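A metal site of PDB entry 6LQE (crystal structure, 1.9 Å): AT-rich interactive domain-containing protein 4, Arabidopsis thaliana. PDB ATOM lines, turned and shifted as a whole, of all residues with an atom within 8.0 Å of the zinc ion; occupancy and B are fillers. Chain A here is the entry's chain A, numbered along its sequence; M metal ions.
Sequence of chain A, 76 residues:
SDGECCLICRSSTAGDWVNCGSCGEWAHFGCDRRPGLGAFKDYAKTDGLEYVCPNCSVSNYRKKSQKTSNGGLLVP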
ATOM      1  N   CYS A   5      21.918 -17.439  27.575  1.00  0.00           N
ATOM      2  CA  CYS A   5      21.588 -16.185  26.890  1.00  0.00           C
ATOM      3  C   CYS A   5      21.459 -16.339  25.386  1.00  0.00           C
ATOM      4  O   CYS A   5      21.736 -17.403  24.827  1.00  0.00           O
ATOM      5  CB  CYS A   5      22.633 -15.117  27.207  1.00  0.00           C
ATOM      6  SG  CYS A   5      24.304 -15.652  26.843  1.00  0.00           S
ATOM      7  N   CYS A   6      21.050 -15.253  24.729  1.00  0.00           N
ATOM      8  CA  CYS A   6      20.707 -15.268  23.305  1.00  0.00           C
ATOM      9  C   CYS A   6      21.899 -15.659  22.434  1.00  0.00           C
ATOM     10  O   CYS A   6      22.940 -15.010  22.501  1.00  0.00           O
ATOM     11  CB  CYS A   6      20.170 -13.894  22.870  1.00  0.00           C
ATOM     12  SG  CYS A   6      19.714 -13.771  21.131  1.00  0.00           S
ATOM     13  N   LEU A   7      21.740 -16.690  21.612  1.00  0.00           N
ATOM     14  CA  LEU A   7      22.857 -17.167  20.798  1.00  0.00           C
ATOM     15  C   LEU A   7      23.268 -16.120  19.766  1.00  0.00           C
ATOM     16  O   LEU A   7      24.349 -16.217  19.185  1.00  0.00           O
ATOM     17  CB  LEU A   7      22.490 -18.515  20.117  1.00  0.00           C
ATOM     18  CG  LEU A   7      21.386 -18.558  19.053  1.00  0.00           C
ATOM     19  CD1 LEU A   7      21.954 -18.350  17.676  1.00  0.00           C
ATOM     20  CD2 LEU A   7      20.617 -19.878  19.089  1.00  0.00           C
ATOM     21  N   ILE A   8      22.410 -15.127  19.516  1.00  0.00           N
ATOM     22  CA  ILE A   8      22.707 -14.075  18.555  1.00  0.00           C
ATOM     23  C   ILE A   8      23.299 -12.804  19.196  1.00  0.00           C
ATOM     24  O   ILE A   8      24.357 -12.350  18.767  1.00  0.00           O
ATOM     25  CB  ILE A   8      21.450 -13.679  17.735  1.00  0.00           C
ATOM     26  CG1 ILE A   8      20.965 -14.881  16.908  1.00  0.00           C
ATOM     27  CG2 ILE A   8      21.731 -12.471  16.834  1.00  0.00           C
ATOM     28  CD1 ILE A   8      19.617 -14.680  16.262  1.00  0.00           C
ATOM     29  N   CYS A   9      22.647 -12.249  20.220  1.00  0.00           N
ATOM     30  CA  CYS A   9      23.096 -10.983  20.814  1.00  0.00           C
ATOM     31  C   CYS A   9      23.809 -11.153  22.156  1.00  0.00           C
ATOM     32  O   CYS A   9      24.417 -10.218  22.650  1.00  0.00           O
ATOM     33  CB  CYS A   9      21.911 -10.025  20.981  1.00  0.00           C
ATOM     34  SG  CYS A   9      20.786 -10.362  22.370  1.00  0.00           S
ATOM     35  N   ARG A  10      23.717 -12.358  22.713  1.00  0.00           N
ATOM     36  CA  ARG A  10      24.405 -12.766  23.945  1.00  0.00           C
ATOM     37  C   ARG A  10      23.955 -12.010  25.201  1.00  0.00           C
ATOM     38  O   ARG A  10      24.684 -11.968  26.197  1.00  0.00           O
ATOM     39  CB  ARG A  10      25.938 -12.624  23.786  1.00  0.00           C
ATOM     40  CG  ARG A  10      26.583 -13.647  22.839  1.00  0.00           C
ATOM     41  CD  ARG A  10      26.614 -15.051  23.458  1.00  0.00           C
ATOM     42  NE  ARG A  10      27.608 -15.133  24.532  1.00  0.00           N
ATOM     43  CZ  ARG A  10      27.691 -16.138  25.406  1.00  0.00           C
ATOM     44  NH1 ARG A  10      26.847 -17.164  25.343  1.00  0.00           N
ATOM     45  NH2 ARG A  10      28.630 -16.122  26.354  1.00  0.00           N
ATOM     46  N   SER A  11      22.770 -11.434  25.170  1.00  0.00           N
ATOM     47  CA  SER A  11      22.169 -10.908  26.377  1.00  0.00           C
ATOM     48  C   SER A  11      21.055 -11.848  26.840  1.00  0.00           C
ATOM     49  O   SER A  11      20.720 -12.806  26.135  1.00  0.00           O
ATOM     50  CB  SER A  11      21.601  -9.518  26.129  1.00  0.00           C
ATOM     51  OG  SER A  11      20.318  -9.645  25.545  1.00  0.00           O
ATOM     52  N   SER A  12      20.477 -11.587  28.006  1.00  0.00           N
ATOM     53  CA  SER A  12      19.327 -12.354  28.454  1.00  0.00           C
ATOM     54  C   SER A  12      18.145 -11.436  28.754  1.00  0.00           C
ATOM     55  O   SER A  12      17.366 -11.707  29.660  1.00  0.00           O
ATOM     56  CB  SER A  12      19.689 -13.190  29.674  1.00  0.00           C
ATOM     57  OG  SER A  12      20.477 -12.404  30.555  1.00  0.00           O
ATOM     58  N   THR A  13      18.023 -10.365  27.987  1.00  0.00           N
ATOM     59  CA  THR A  13      16.947  -9.395  28.185  1.00  0.00           C
ATOM     60  C   THR A  13      15.575 -10.037  27.934  1.00  0.00           C
ATOM     61  O   THR A  13      15.489 -11.091  27.291  1.00  0.00           O
ATOM     62  CB  THR A  13      17.123  -8.170  27.268  1.00  0.00           C
ATOM     63  OG1 THR A  13      17.055  -8.584  25.897  1.00  0.00           O
ATOM     64  CG2 THR A  13      18.460  -7.499  27.514  1.00  0.00           C
ATOM     65  N   ALA A  14      14.510  -9.408  28.420  1.00  0.00           N
ATOM     66  CA  ALA A  14      13.138  -9.885  28.240  1.00  0.00           C
ATOM     67  C   ALA A  14      12.710  -9.928  26.771  1.00  0.00           C
ATOM     68  O   ALA A  14      13.190  -9.136  25.950  1.00  0.00           O
ATOM     69  CB  ALA A  14      12.176  -9.027  29.014  1.00  0.00           C
ATOM     70  N   ASP A  16      10.619 -12.518  23.414  1.00  0.00           N
ATOM     71  CA  ASP A  16      10.131 -13.777  22.878  1.00  0.00           C
ATOM     72  C   ASP A  16      11.293 -14.663  22.476  1.00  0.00           C
ATOM     73  O   ASP A  16      12.112 -14.294  21.637  1.00  0.00           O
ATOM     74  CB  ASP A  16       9.201 -13.544  21.683  1.00  0.00           C
ATOM     75  CG  ASP A  16       7.905 -12.856  22.056  1.00  0.00           C
ATOM     76  OD1 ASP A  16       7.590 -12.756  23.262  1.00  0.00           O
ATOM     77  OD2 ASP A  16       7.202 -12.402  21.134  1.00  0.00           O
ATOM     78  N   TRP A  17      11.356 -15.845  23.058  1.00  0.00           N
ATOM     79  CA  TRP A  17      12.505 -16.715  22.876  1.00  0.00           C
ATOM     80  C   TRP A  17      12.154 -17.984  22.133  1.00  0.00           C
ATOM     81  O   TRP A  17      11.123 -18.589  22.393  1.00  0.00           O
ATOM     82  CB  TRP A  17      13.096 -17.102  24.228  1.00  0.00           C
ATOM     83  CG  TRP A  17      13.707 -16.015  25.031  1.00  0.00           C
ATOM     84  CD1 TRP A  17      13.067 -15.043  25.734  1.00  0.00           C
ATOM     85  CD2 TRP A  17      15.105 -15.821  25.268  1.00  0.00           C
ATOM     86  NE1 TRP A  17      13.974 -14.239  26.379  1.00  0.00           N
ATOM     87  CE2 TRP A  17      15.237 -14.697  26.110  1.00  0.00           C
ATOM     88  CE3 TRP A  17      16.261 -16.470  24.837  1.00  0.00           C
ATOM     89  CZ2 TRP A  17      16.474 -14.226  26.538  1.00  0.00           C
ATOM     90  CZ3 TRP A  17      17.488 -16.002  25.273  1.00  0.00           C
ATOM     91  CH2 TRP A  17      17.580 -14.894  26.106  1.00  0.00           C
ATOM     92  N   TRP A  26      19.308 -21.106  22.960  1.00  0.00           N
ATOM     93  CA  TRP A  26      18.174 -20.178  22.856  1.00  0.00           C
ATOM     94  C   TRP A  26      18.523 -18.900  22.099  1.00  0.00           C
ATOM     95  O   TRP A  26      19.680 -18.512  22.043  1.00  0.00           O
ATOM     96  CB  TRP A  26      17.669 -19.789  24.243  1.00  0.00           C
ATOM     97  CG  TRP A  26      16.975 -20.877  24.992  1.00  0.00           C
ATOM     98  CD1 TRP A  26      17.542 -21.754  25.867  1.00  0.00           C
ATOM     99  CD2 TRP A  26      15.575 -21.172  24.970  1.00  0.00           C
ATOM    100  NE1 TRP A  26      16.579 -22.585  26.384  1.00  0.00           N
ATOM    101  CE2 TRP A  26      15.370 -22.249  25.847  1.00  0.00           C
ATOM    102  CE3 TRP A  26      14.484 -20.643  24.290  1.00  0.00           C
ATOM    103  CZ2 TRP A  26      14.105 -22.810  26.052  1.00  0.00           C
ATOM    104  CZ3 TRP A  26      13.236 -21.188  24.500  1.00  0.00           C
ATOM    105  CH2 TRP A  26      13.055 -22.259  25.374  1.00  0.00           C
ATOM    106  N   ALA A  27      17.510 -18.259  21.537  1.00  0.00           N
ATOM    107  CA  ALA A  27      17.690 -16.986  20.862  1.00  0.00           C
ATOM    108  C   ALA A  27      16.431 -16.135  21.019  1.00  0.00           C
ATOM    109  O   ALA A  27      15.328 -16.687  21.058  1.00  0.00           O
ATOM    110  CB  ALA A  27      17.998 -17.208  19.380  1.00  0.00           C
ATOM    111  N   HIS A  28      16.573 -14.807  21.141  1.00  0.00           N
ATOM    112  CA  HIS A  28      15.405 -13.933  20.973  1.00  0.00           C
ATOM    113  C   HIS A  28      14.887 -14.101  19.560  1.00  0.00           C
ATOM    114  O   HIS A  28      15.653 -13.960  18.617  1.00  0.00           O
ATOM    115  CB  HIS A  28      15.735 -12.465  21.173  1.00  0.00           C
ATOM    116  CG  HIS A  28      16.273 -12.122  22.525  1.00  0.00           C
ATOM    117  ND1 HIS A  28      17.557 -11.673  22.704  1.00  0.00           N
ATOM    118  CD2 HIS A  28      15.690 -12.110  23.750  1.00  0.00           C
ATOM    119  CE1 HIS A  28      17.766 -11.416  23.993  1.00  0.00           C
ATOM    120  NE2 HIS A  28      16.643 -11.675  24.644  1.00  0.00           N
ATOM    121  N   PHE A  29      13.597 -14.352  19.414  1.00  0.00           N
ATOM    122  CA  PHE A  29      13.029 -14.465  18.080  1.00  0.00           C
ATOM    123  C   PHE A  29      13.235 -13.147  17.295  1.00  0.00           C
ATOM    124  O   PHE A  29      13.500 -13.146  16.086  1.00  0.00           O
ATOM    125  CB  PHE A  29      11.543 -14.820  18.169  1.00  0.00           C
ATOM    126  CG  PHE A  29      10.938 -15.161  16.852  1.00  0.00           C
ATOM    127  CD1 PHE A  29      11.166 -16.380  16.282  1.00  0.00           C
ATOM    128  CD2 PHE A  29      10.183 -14.230  16.174  1.00  0.00           C
ATOM    129  CE1 PHE A  29      10.639 -16.706  15.052  1.00  0.00           C
ATOM    130  CE2 PHE A  29       9.650 -14.539  14.932  1.00  0.00           C
ATOM    131  CZ  PHE A  29       9.874 -15.779  14.383  1.00  0.00           C
ATOM    132  N   GLY A  30      13.141 -12.019  17.984  1.00  0.00           N
ATOM    133  CA  GLY A  30      13.364 -10.740  17.352  1.00  0.00           C
ATOM    134  C   GLY A  30      14.782 -10.452  16.858  1.00  0.00           C
ATOM    135  O   GLY A  30      14.955  -9.574  16.027  1.00  0.00           O
ATOM    136  N   CYS A  31      15.785 -11.186  17.334  1.00  0.00           N
ATOM    137  CA  CYS A  31      17.164 -10.966  16.878  1.00  0.00           C
ATOM    138  C   CYS A  31      17.488 -11.680  15.568  1.00  0.00           C
ATOM    139  O   CYS A  31      18.478 -11.364  14.910  1.00  0.00           O
ATOM    140  CB  CYS A  31      18.162 -11.412  17.949  1.00  0.00           C
ATOM    141  SG  CYS A  31      18.267 -10.333  19.398  1.00  0.00           S
ATOM    142  N   ASP A  32      16.672 -12.667  15.216  1.00  0.00           N
ATOM    143  CA  ASP A  32      16.828 -13.402  13.971  1.00  0.00           C
ATOM    144  C   ASP A  32      16.024 -12.734  12.862  1.00  0.00           C
ATOM    145  O   ASP A  32      14.791 -12.789  12.844  1.00  0.00           O
ATOM    146  CB  ASP A  32      16.398 -14.838  14.167  1.00  0.00           C
ATOM    147  CG  ASP A  32      16.884 -15.745  13.035  1.00  0.00           C
ATOM    148  OD1 ASP A  32      17.232 -15.240  11.947  1.00  0.00           O
ATOM    149  OD2 ASP A  32      16.901 -16.957  13.255  1.00  0.00           O
HETATM  150 ZN    ZN M   1      19.161 -11.571  21.417  1.00  0.00          ZN
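A ring nitrogen (ND1) of His 28 binds the zinc ion (2.1 Å).
The zinc ion is bound by the side-chain sulfur (SG) of Cys 9, 2.2 Å away.
SG of Cys 6 is bound to the zinc ion, at 2.3 Å.
The zinc ion is bound by SG of Cys 31.
The zinc ion has four donor atoms within binding distance.
The side-chain sulfur (SG) of Cys 6 lies close to the backbone NH (N) of Ile 8 (3.4 Å).
SG of Cys 9 sits close to OG of Ser 11 (3.3 Å).
NE2 of His 28 is in hydrogen-bond range of O of Thr 13 (2.9 Å).
The backbone NH (N) of Cys 6 is in hydrogen-bond range of the backbone carbonyl oxygen (O) of Ser 11, 2.8 Å away.
Of the 19 residues printed, 4 come within 4 Å of the zinc ion.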
